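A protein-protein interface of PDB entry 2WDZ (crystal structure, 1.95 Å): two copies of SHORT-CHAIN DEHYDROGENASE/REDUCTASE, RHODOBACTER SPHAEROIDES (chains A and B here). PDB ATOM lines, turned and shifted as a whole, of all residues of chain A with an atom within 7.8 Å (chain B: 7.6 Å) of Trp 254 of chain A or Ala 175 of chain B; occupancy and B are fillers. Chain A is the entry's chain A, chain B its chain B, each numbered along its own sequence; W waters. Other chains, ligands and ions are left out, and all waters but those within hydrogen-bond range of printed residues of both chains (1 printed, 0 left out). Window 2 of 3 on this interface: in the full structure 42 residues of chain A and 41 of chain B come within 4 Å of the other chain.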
ATOM      1  N   ILE A 149       4.103 -24.866  -1.926  1.00  0.00           N
ATOM      2  CA  ILE A 149       3.661 -24.692  -3.338  1.00  0.00           C
ATOM      3  C   ILE A 149       4.366 -25.753  -4.217  1.00  0.00           C
ATOM      4  O   ILE A 149       5.103 -26.615  -3.678  1.00  0.00           O
ATOM      5  CB  ILE A 149       3.972 -23.271  -3.846  1.00  0.00           C
ATOM      6  CG1 ILE A 149       5.480 -23.015  -3.827  1.00  0.00           C
ATOM      7  CG2 ILE A 149       3.240 -22.234  -3.008  1.00  0.00           C
ATOM      8  CD1 ILE A 149       6.143 -23.169  -5.177  1.00  0.00           C
ATOM      9  N   THR A 209      12.200 -18.545 -16.049  1.00  0.00           N
ATOM     10  CA  THR A 209      10.954 -18.716 -15.313  1.00  0.00           C
ATOM     11  C   THR A 209      11.185 -18.600 -13.810  1.00  0.00           C
ATOM     12  O   THR A 209      10.383 -17.963 -13.115  1.00  0.00           O
ATOM     13  CB  THR A 209      10.269 -20.059 -15.632  1.00  0.00           C
ATOM     14  OG1 THR A 209       9.940 -20.097 -17.026  1.00  0.00           O
ATOM     15  CG2 THR A 209       8.983 -20.256 -14.813  1.00  0.00           C
ATOM     16  N   TRP A 210      12.266 -19.215 -13.319  1.00  0.00           N
ATOM     17  CA  TRP A 210      12.599 -19.189 -11.876  1.00  0.00           C
ATOM     18  C   TRP A 210      12.673 -17.756 -11.335  1.00  0.00           C
ATOM     19  O   TRP A 210      11.995 -17.425 -10.341  1.00  0.00           O
ATOM     20  CB  TRP A 210      13.902 -19.931 -11.594  1.00  0.00           C
ATOM     21  CG  TRP A 210      13.819 -21.430 -11.779  1.00  0.00           C
ATOM     22  CD1 TRP A 210      12.817 -22.150 -12.407  1.00  0.00           C
ATOM     23  CD2 TRP A 210      14.772 -22.374 -11.337  1.00  0.00           C
ATOM     24  NE1 TRP A 210      13.105 -23.496 -12.368  1.00  0.00           N
ATOM     25  CE2 TRP A 210      14.309 -23.657 -11.721  1.00  0.00           C
ATOM     26  CE3 TRP A 210      15.998 -22.271 -10.657  1.00  0.00           C
ATOM     27  CZ2 TRP A 210      15.037 -24.826 -11.440  1.00  0.00           C
ATOM     28  CZ3 TRP A 210      16.705 -23.446 -10.369  1.00  0.00           C
ATOM     29  CH2 TRP A 210      16.219 -24.695 -10.752  1.00  0.00           C
ATOM     30  N   LEU A 211      13.425 -16.910 -12.032  1.00  0.00           N
ATOM     31  CA  LEU A 211      13.676 -15.545 -11.572  1.00  0.00           C
ATOM     32  C   LEU A 211      12.438 -14.688 -11.732  1.00  0.00           C
ATOM     33  O   LEU A 211      12.083 -13.900 -10.860  1.00  0.00           O
ATOM     34  CB  LEU A 211      14.855 -14.928 -12.314  1.00  0.00           C
ATOM     35  CG  LEU A 211      16.174 -15.705 -12.282  1.00  0.00           C
ATOM     36  CD1 LEU A 211      17.216 -15.126 -13.228  1.00  0.00           C
ATOM     37  CD2 LEU A 211      16.730 -15.800 -10.869  1.00  0.00           C
ATOM     38  N   ASP A 212      11.744 -14.886 -12.836  1.00  0.00           N
ATOM     39  CA  ASP A 212      10.499 -14.180 -13.074  1.00  0.00           C
ATOM     40  C   ASP A 212       9.470 -14.363 -11.992  1.00  0.00           C
ATOM     41  O   ASP A 212       8.711 -13.439 -11.735  1.00  0.00           O
ATOM     42  CB  ASP A 212       9.872 -14.623 -14.391  1.00  0.00           C
ATOM     43  CG  ASP A 212       9.464 -13.461 -15.223  1.00  0.00           C
ATOM     44  OD1 ASP A 212      10.361 -12.884 -15.893  1.00  0.00           O
ATOM     45  OD2 ASP A 212       8.266 -13.087 -15.176  1.00  0.00           O
ATOM     46  N   MET A 213       9.435 -15.578 -11.426  1.00  0.00           N
ATOM     47  CA  MET A 213       8.509 -16.022 -10.381  1.00  0.00           C
ATOM     48  C   MET A 213       8.991 -15.582  -8.990  1.00  0.00           C
ATOM     49  O   MET A 213       8.291 -15.737  -7.986  1.00  0.00           O
ATOM     50  CB  MET A 213       8.401 -17.538 -10.427  1.00  0.00           C
ATOM     51  CG  MET A 213       7.608 -18.117 -11.618  1.00  0.00           C
ATOM     52  SD  MET A 213       5.881 -17.686 -11.418  1.00  0.00           S
ATOM     53  CE  MET A 213       5.273 -18.809 -10.140  1.00  0.00           C
ATOM     54  N   THR A 214      10.218 -15.066  -8.944  1.00  0.00           N
ATOM     55  CA  THR A 214      10.824 -14.615  -7.694  1.00  0.00           C
ATOM     56  C   THR A 214      10.835 -13.066  -7.591  1.00  0.00           C
ATOM     57  O   THR A 214      11.561 -12.412  -8.340  1.00  0.00           O
ATOM     58  CB  THR A 214      12.228 -15.226  -7.534  1.00  0.00           C
ATOM     59  OG1 THR A 214      12.093 -16.658  -7.600  1.00  0.00           O
ATOM     60  CG2 THR A 214      12.859 -14.837  -6.193  1.00  0.00           C
ATOM     61  N   PRO A 215      10.021 -12.497  -6.665  1.00  0.00           N
ATOM     62  CA  PRO A 215       9.943 -11.052  -6.470  1.00  0.00           C
ATOM     63  C   PRO A 215      11.330 -10.440  -6.364  1.00  0.00           C
ATOM     64  O   PRO A 215      11.578  -9.405  -6.960  1.00  0.00           O
ATOM     65  CB  PRO A 215       9.191 -10.951  -5.136  1.00  0.00           C
ATOM     66  CG  PRO A 215       8.213 -12.123  -5.227  1.00  0.00           C
ATOM     67  CD  PRO A 215       9.125 -13.200  -5.715  1.00  0.00           C
ATOM     68  N   MET A 216      12.219 -11.032  -5.575  1.00  0.00           N
ATOM     69  CA  MET A 216      13.586 -10.473  -5.478  1.00  0.00           C
ATOM     70  C   MET A 216      14.432 -10.580  -6.775  1.00  0.00           C
ATOM     71  O   MET A 216      15.548 -10.026  -6.843  1.00  0.00           O
ATOM     72  CB  MET A 216      14.338 -11.067  -4.279  1.00  0.00           C
ATOM     73  CG  MET A 216      14.034 -10.410  -2.978  1.00  0.00           C
ATOM     74  SD  MET A 216      15.129 -10.878  -1.622  1.00  0.00           S
ATOM     75  CE  MET A 216      16.534  -9.864  -1.992  1.00  0.00           C
ATOM     76  N   GLY A 217      13.894 -11.287  -7.774  1.00  0.00           N
ATOM     77  CA  GLY A 217      14.529 -11.478  -9.092  1.00  0.00           C
ATOM     78  C   GLY A 217      15.892 -12.175  -9.083  1.00  0.00           C
ATOM     79  O   GLY A 217      16.717 -11.935  -9.971  1.00  0.00           O
ATOM     80  N   GLY A 249      12.995 -15.297  -1.172  1.00  0.00           N
ATOM     81  CA  GLY A 249      13.022 -14.109  -2.003  1.00  0.00           C
ATOM     82  C   GLY A 249      11.627 -13.617  -2.396  1.00  0.00           C
ATOM     83  O   GLY A 249      11.459 -12.870  -3.391  1.00  0.00           O
ATOM     84  N   GLY A 250      10.633 -14.041  -1.596  1.00  0.00           N
ATOM     85  CA  GLY A 250       9.226 -13.720  -1.795  1.00  0.00           C
ATOM     86  C   GLY A 250       8.493 -14.752  -2.668  1.00  0.00           C
ATOM     87  O   GLY A 250       7.379 -14.520  -3.081  1.00  0.00           O
ATOM     88  N   TYR A 251       9.130 -15.875  -2.972  1.00  0.00           N
ATOM     89  CA  TYR A 251       8.547 -16.700  -3.986  1.00  0.00           C
ATOM     90  C   TYR A 251       7.116 -17.139  -3.647  1.00  0.00           C
ATOM     91  O   TYR A 251       6.232 -17.084  -4.526  1.00  0.00           O
ATOM     92  CB  TYR A 251       9.406 -17.921  -4.215  1.00  0.00           C
ATOM     93  CG  TYR A 251       8.941 -18.764  -5.374  1.00  0.00           C
ATOM     94  CD1 TYR A 251       9.578 -18.623  -6.630  1.00  0.00           C
ATOM     95  CD2 TYR A 251       7.897 -19.706  -5.250  1.00  0.00           C
ATOM     96  CE1 TYR A 251       9.173 -19.378  -7.730  1.00  0.00           C
ATOM     97  CE2 TYR A 251       7.492 -20.501  -6.382  1.00  0.00           C
ATOM     98  CZ  TYR A 251       8.157 -20.318  -7.593  1.00  0.00           C
ATOM     99  OH  TYR A 251       7.838 -21.048  -8.664  1.00  0.00           O
ATOM    100  N   THR A 252       6.907 -17.579  -2.394  1.00  0.00           N
ATOM    101  CA  THR A 252       5.578 -18.042  -1.949  1.00  0.00           C
ATOM    102  C   THR A 252       4.573 -16.899  -1.718  1.00  0.00           C
ATOM    103  O   THR A 252       3.405 -17.171  -1.431  1.00  0.00           O
ATOM    104  CB  THR A 252       5.604 -18.965  -0.688  1.00  0.00           C
ATOM    105  OG1 THR A 252       6.202 -18.289   0.419  1.00  0.00           O
ATOM    106  CG2 THR A 252       6.414 -20.210  -0.949  1.00  0.00           C
ATOM    107  N   VAL A 253       5.029 -15.647  -1.879  1.00  0.00           N
ATOM    108  CA  VAL A 253       4.126 -14.475  -1.836  1.00  0.00           C
ATOM    109  C   VAL A 253       3.152 -14.341  -3.045  1.00  0.00           C
ATOM    110  O   VAL A 253       1.974 -14.075  -2.860  1.00  0.00           O
ATOM    111  CB  VAL A 253       4.934 -13.166  -1.589  1.00  0.00           C
ATOM    112  CG1 VAL A 253       4.034 -11.980  -1.493  1.00  0.00           C
ATOM    113  CG2 VAL A 253       5.740 -13.339  -0.310  1.00  0.00           C
ATOM    114  N   TRP A 254       3.669 -14.511  -4.265  1.00  0.00           N
ATOM    115  CA  TRP A 254       2.850 -14.560  -5.463  1.00  0.00           C
ATOM    116  C   TRP A 254       2.062 -15.837  -5.662  1.00  0.00           C
ATOM    117  O   TRP A 254       1.001 -15.845  -6.268  1.00  0.00           O
ATOM    118  CB  TRP A 254       3.737 -14.434  -6.676  1.00  0.00           C
ATOM    119  CG  TRP A 254       4.135 -13.043  -6.898  1.00  0.00           C
ATOM    120  CD1 TRP A 254       3.491 -11.939  -6.452  1.00  0.00           C
ATOM    121  CD2 TRP A 254       5.284 -12.599  -7.607  1.00  0.00           C
ATOM    122  NE1 TRP A 254       4.162 -10.802  -6.861  1.00  0.00           N
ATOM    123  CE2 TRP A 254       5.267 -11.187  -7.586  1.00  0.00           C
ATOM    124  CE3 TRP A 254       6.320 -13.256  -8.278  1.00  0.00           C
ATOM    125  CZ2 TRP A 254       6.265 -10.409  -8.207  1.00  0.00           C
ATOM    126  CZ3 TRP A 254       7.293 -12.490  -8.924  1.00  0.00           C
ATOM    127  CH2 TRP A 254       7.271 -11.080  -8.860  1.00  0.00           C
ATOM    128  OXT TRP A 254       2.545 -16.887  -5.273  1.00  0.00           O
ATOM    129  N   GLN B 168      -1.349 -10.000   5.490  1.00  0.00           N
ATOM    130  CA  GLN B 168      -1.454  -9.836   4.036  1.00  0.00           C
ATOM    131  C   GLN B 168      -0.933  -8.488   3.470  1.00  0.00           C
ATOM    132  O   GLN B 168      -0.393  -8.450   2.372  1.00  0.00           O
ATOM    133  CB  GLN B 168      -2.866 -10.063   3.535  1.00  0.00           C
ATOM    134  CG  GLN B 168      -3.270 -11.494   3.276  1.00  0.00           C
ATOM    135  CD  GLN B 168      -2.424 -12.141   2.184  1.00  0.00           C
ATOM    136  OE1 GLN B 168      -2.678 -11.967   0.977  1.00  0.00           O
ATOM    137  NE2 GLN B 168      -1.445 -12.893   2.595  1.00  0.00           N
ATOM    138  N   LEU B 169      -1.115  -7.417   4.234  1.00  0.00           N
ATOM    139  CA  LEU B 169      -0.423  -6.167   4.047  1.00  0.00           C
ATOM    140  C   LEU B 169       1.081  -6.382   3.960  1.00  0.00           C
ATOM    141  O   LEU B 169       1.722  -5.887   3.063  1.00  0.00           O
ATOM    142  CB  LEU B 169      -0.774  -5.148   5.173  1.00  0.00           C
ATOM    143  CG  LEU B 169      -0.130  -3.729   5.013  1.00  0.00           C
ATOM    144  CD1 LEU B 169      -0.625  -2.723   5.935  1.00  0.00           C
ATOM    145  CD2 LEU B 169       1.370  -3.811   5.207  1.00  0.00           C
ATOM    146  N   THR B 170       1.638  -7.128   4.906  1.00  0.00           N
ATOM    147  CA  THR B 170       3.039  -7.489   4.887  1.00  0.00           C
ATOM    148  C   THR B 170       3.466  -8.073   3.550  1.00  0.00           C
ATOM    149  O   THR B 170       4.364  -7.560   2.882  1.00  0.00           O
ATOM    150  CB  THR B 170       3.353  -8.454   6.052  1.00  0.00           C
ATOM    151  OG1 THR B 170       3.054  -7.791   7.259  1.00  0.00           O
ATOM    152  CG2 THR B 170       4.796  -8.897   6.068  1.00  0.00           C
ATOM    153  N   ARG B 171       2.751  -9.094   3.128  1.00  0.00           N
ATOM    154  CA  ARG B 171       3.021  -9.766   1.851  1.00  0.00           C
ATOM    155  C   ARG B 171       2.826  -8.890   0.641  1.00  0.00           C
ATOM    156  O   ARG B 171       3.691  -8.922  -0.265  1.00  0.00           O
ATOM    157  CB  ARG B 171       2.192 -11.051   1.821  1.00  0.00           C
ATOM    158  CG  ARG B 171       2.741 -11.920   2.966  1.00  0.00           C
ATOM    159  CD  ARG B 171       1.808 -12.914   3.403  1.00  0.00           C
ATOM    160  NE  ARG B 171       1.411 -13.759   2.305  1.00  0.00           N
ATOM    161  CZ  ARG B 171       2.089 -14.805   1.843  1.00  0.00           C
ATOM    162  NH1 ARG B 171       3.292 -15.127   2.370  1.00  0.00           N
ATOM    163  NH2 ARG B 171       1.566 -15.522   0.828  1.00  0.00           N
ATOM    164  N   ALA B 172       1.772  -8.048   0.672  1.00  0.00           N
ATOM    165  CA  ALA B 172       1.439  -7.118  -0.460  1.00  0.00           C
ATOM    166  C   ALA B 172       2.568  -6.082  -0.688  1.00  0.00           C
ATOM    167  O   ALA B 172       3.000  -5.889  -1.826  1.00  0.00           O
ATOM    168  CB  ALA B 172       0.103  -6.419  -0.270  1.00  0.00           C
ATOM    169  N   LEU B 173       3.052  -5.450   0.393  1.00  0.00           N
ATOM    170  CA  LEU B 173       4.193  -4.519   0.301  1.00  0.00           C
ATOM    171  C   LEU B 173       5.534  -5.259  -0.030  1.00  0.00           C
ATOM    172  O   LEU B 173       6.350  -4.782  -0.857  1.00  0.00           O
ATOM    173  CB  LEU B 173       4.302  -3.654   1.546  1.00  0.00           C
ATOM    174  CG  LEU B 173       3.101  -2.780   2.030  1.00  0.00           C
ATOM    175  CD1 LEU B 173       3.470  -1.864   3.211  1.00  0.00           C
ATOM    176  CD2 LEU B 173       2.664  -1.942   0.835  1.00  0.00           C
ATOM    177  N   ALA B 174       5.735  -6.427   0.560  1.00  0.00           N
ATOM    178  CA  ALA B 174       6.911  -7.267   0.186  1.00  0.00           C
ATOM    179  C   ALA B 174       6.911  -7.494  -1.323  1.00  0.00           C
ATOM    180  O   ALA B 174       7.928  -7.330  -1.992  1.00  0.00           O
ATOM    181  CB  ALA B 174       6.854  -8.602   0.871  1.00  0.00           C
ATOM    182  N   ALA B 175       5.770  -7.885  -1.862  1.00  0.00           N
ATOM    183  CA  ALA B 175       5.749  -8.180  -3.321  1.00  0.00           C
ATOM    184  C   ALA B 175       5.973  -6.906  -4.155  1.00  0.00           C
ATOM    185  O   ALA B 175       6.713  -6.912  -5.175  1.00  0.00           O
ATOM    186  CB  ALA B 175       4.461  -8.854  -3.751  1.00  0.00           C
ATOM    187  N   GLU B 176       5.348  -5.820  -3.701  1.00  0.00           N
ATOM    188  CA  GLU B 176       5.401  -4.556  -4.442  1.00  0.00           C
ATOM    189  C   GLU B 176       6.807  -3.879  -4.484  1.00  0.00           C
ATOM    190  O   GLU B 176       7.190  -3.324  -5.516  1.00  0.00           O
ATOM    191  CB  GLU B 176       4.280  -3.611  -3.955  1.00  0.00           C
ATOM    192  CG  GLU B 176       4.201  -2.226  -4.689  1.00  0.00           C
ATOM    193  CD  GLU B 176       2.832  -1.501  -4.453  1.00  0.00           C
ATOM    194  OE1 GLU B 176       1.943  -1.994  -3.664  1.00  0.00           O
ATOM    195  OE2 GLU B 176       2.649  -0.431  -5.045  1.00  0.00           O
ATOM    196  N   TRP B 177       7.556  -3.944  -3.372  1.00  0.00           N
ATOM    197  CA  TRP B 177       8.826  -3.303  -3.239  1.00  0.00           C
ATOM    198  C   TRP B 177      10.053  -4.242  -3.305  1.00  0.00           C
ATOM    199  O   TRP B 177      11.189  -3.804  -3.106  1.00  0.00           O
ATOM    200  CB  TRP B 177       8.854  -2.499  -1.941  1.00  0.00           C
ATOM    201  CG  TRP B 177       7.824  -1.401  -1.872  1.00  0.00           C
ATOM    202  CD1 TRP B 177       7.199  -0.766  -2.929  1.00  0.00           C
ATOM    203  CD2 TRP B 177       7.329  -0.786  -0.696  1.00  0.00           C
ATOM    204  NE1 TRP B 177       6.335   0.172  -2.464  1.00  0.00           N
ATOM    205  CE2 TRP B 177       6.382   0.174  -1.095  1.00  0.00           C
ATOM    206  CE3 TRP B 177       7.578  -0.971   0.675  1.00  0.00           C
ATOM    207  CZ2 TRP B 177       5.735   1.006  -0.186  1.00  0.00           C
ATOM    208  CZ3 TRP B 177       6.877  -0.186   1.585  1.00  0.00           C
ATOM    209  CH2 TRP B 177       5.973   0.792   1.155  1.00  0.00           C
ATOM    210  N   ALA B 178       9.814  -5.524  -3.556  1.00  0.00           N
ATOM    211  CA  ALA B 178      10.893  -6.534  -3.622  1.00  0.00           C
ATOM    212  C   ALA B 178      11.943  -6.146  -4.643  1.00  0.00           C
ATOM    213  O   ALA B 178      13.135  -6.221  -4.375  1.00  0.00           O
ATOM    214  CB  ALA B 178      10.319  -7.857  -4.022  1.00  0.00           C
ATOM    215  N   GLY B 179      11.459  -5.784  -5.833  1.00  0.00           N
ATOM    216  CA  GLY B 179      12.284  -5.432  -6.971  1.00  0.00           C
ATOM    217  C   GLY B 179      13.090  -4.188  -6.741  1.00  0.00           C
ATOM    218  O   GLY B 179      14.092  -3.986  -7.434  1.00  0.00           O
ATOM    219  N   ARG B 180      12.663  -3.376  -5.762  1.00  0.00           N
ATOM    220  CA  ARG B 180      13.283  -2.109  -5.425  1.00  0.00           C
ATOM    221  C   ARG B 180      13.976  -2.139  -4.088  1.00  0.00           C
ATOM    222  O   ARG B 180      14.234  -1.095  -3.502  1.00  0.00           O
ATOM    223  CB  ARG B 180      12.259  -0.976  -5.432  1.00  0.00           C
ATOM    224  CG  ARG B 180      11.894  -0.486  -6.848  1.00  0.00           C
ATOM    225  CD  ARG B 180      10.692   0.474  -6.791  1.00  0.00           C
ATOM    226  NE  ARG B 180       9.407  -0.248  -6.721  1.00  0.00           N
ATOM    227  CZ  ARG B 180       8.218   0.354  -6.746  1.00  0.00           C
ATOM    228  NH1 ARG B 180       8.163   1.678  -6.794  1.00  0.00           N
ATOM    229  NH2 ARG B 180       7.084  -0.345  -6.710  1.00  0.00           N
ATOM    230  N   VAL B 182      13.350  -3.297  -0.942  1.00  0.00           N
ATOM    231  CA  VAL B 182      12.829  -3.220   0.423  1.00  0.00           C
ATOM    232  C   VAL B 182      12.191  -4.557   0.800  1.00  0.00           C
ATOM    233  O   VAL B 182      11.276  -5.028   0.088  1.00  0.00           O
ATOM    234  CB  VAL B 182      11.860  -2.021   0.678  1.00  0.00           C
ATOM    235  CG1 VAL B 182      11.461  -2.029   2.167  1.00  0.00           C
ATOM    236  CG2 VAL B 182      12.515  -0.688   0.237  1.00  0.00           C
ATOM    237  N   VAL B 184      10.006  -6.867   3.514  1.00  0.00           N
ATOM    238  CA  VAL B 184       8.884  -6.643   4.478  1.00  0.00           C
ATOM    239  C   VAL B 184       8.427  -8.009   5.004  1.00  0.00           C
ATOM    240  O   VAL B 184       8.099  -8.889   4.234  1.00  0.00           O
ATOM    241  CB  VAL B 184       7.667  -5.923   3.858  1.00  0.00           C
ATOM    242  CG1 VAL B 184       6.600  -5.584   4.927  1.00  0.00           C
ATOM    243  CG2 VAL B 184       8.080  -4.738   3.035  1.00  0.00           C
ATOM    244  N   THR B 241      11.759 -12.282   2.454  1.00  0.00           N
ATOM    245  CA  THR B 241      10.737 -11.260   2.274  1.00  0.00           C
ATOM    246  C   THR B 241       9.349 -11.834   2.089  1.00  0.00           C
ATOM    247  O   THR B 241       9.193 -12.856   1.419  1.00  0.00           O
ATOM    248  CB  THR B 241      11.058 -10.224   1.110  1.00  0.00           C
ATOM    249  OG1 THR B 241      10.262  -9.034   1.276  1.00  0.00           O
ATOM    250  CG2 THR B 241      10.863 -10.812  -0.312  1.00  0.00           C
ATOM    251  N   GLY B 242       8.364 -11.134   2.661  1.00  0.00           N
ATOM    252  CA  GLY B 242       6.951 -11.543   2.654  1.00  0.00           C
ATOM    253  C   GLY B 242       6.680 -12.755   3.585  1.00  0.00           C
ATOM    254  O   GLY B 242       5.737 -13.484   3.365  1.00  0.00           O
HETATM  255  O   HOH W   1       5.753 -16.493   2.239  1.00  0.00           O
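The backbone carbonyl oxygen (O) of Thr 252 of chain A is in hydrogen-bond range of the guanidinium group (NH2) of Arg 171 of chain B (3.3 Å).
The guanidinium group of Arg 171 of chain B sits close to the side-chain amide nitrogen of Gln 168 of chain B, at 3.0 Å. The backbone carbonyl oxygen (O) of Val 184 of chain B is in hydrogen-bond range of the backbone NH (N) of Gly 242 of chain B, 2.8 Å away. The guanidinium group (NH1) of Arg 171 of chain B lies within hydrogen-bond range of the backbone carbonyl oxygen (O) of Gly 242 of chain B, 3.1 Å away. The backbone NH (N) of Met 216 of chain A lies within hydrogen-bond range of the backbone carbonyl oxygen (O) of Gly 249 of chain A. N of Val 184 of chain B is in hydrogen-bond range of OG1 of Thr 241 of chain B (3.1 Å).
Among the printed residues, merely in contact across the chains: Pro 215 of chain A with Ala 178 of chain B (3.5 Å), Pro 215 of chain A with Gly 179 of chain B (3.8 Å), Gly 249 of chain A with Thr 241 of chain B (3.6 Å), Gly 250 of chain A with Thr 241 of chain B (3.3 Å), Val 253 of chain A with Arg 171 of chain B (3.3 Å), Val 253 of chain A with Ala 175 of chain B (3.9 Å), Val 253 of chain A with Thr 241 of chain B (3.9 Å), Val 253 of chain A with Gly 242 of chain B (3.7 Å) and Trp 254 of chain A with Ala 175 of chain B (3.7 Å).
Trp 254 of chain A touches one residue of chain B. Ala 175 of chain B touches two residues of chain A. No residue of chain A comes within 4 Å of Ala 174 of chain B. Of the printed residues of chain A, Thr 241 of chain B touches Gly 249, Gly 250 and Val 253. Of the printed residues of chain B, Thr 252 of chain A touches Arg 171 (3.3 Å). The nearest residue of chain A that does not touch Ala 175 of chain B is Pro 215 of chain A (4.7 Å).
Of the 16 printed residues of chain A, 6 touch a printed residue of chain B. Printed residues of chain A that touch a printed residue of chain B: Pro 215, Gly 249, Gly 250, Thr 252, Val 253 and Trp 254. Hydrophobic or aromatic side chains of chain A within 4 Å of the printed part of chain B: Pro 215, Val 253 and Trp 254. Hydrophobic or aromatic side chains of chain B that line the printed part of chain A: Ala 175 and Ala 178. Among the printed residues, 10 pairs touch across the chains.
No position is printed for both chains. Of the 10 pairs that touch across the chains among the printed residues, none has its exchanged pair printed and touching as well.
Water W1 lies within hydrogen-bond range of OG1 of Thr 252 of chain A (2.6 Å), NH1 of Arg 171 of chain B (2.8 Å) and O of Gly 242 of chain B (3.2 Å).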
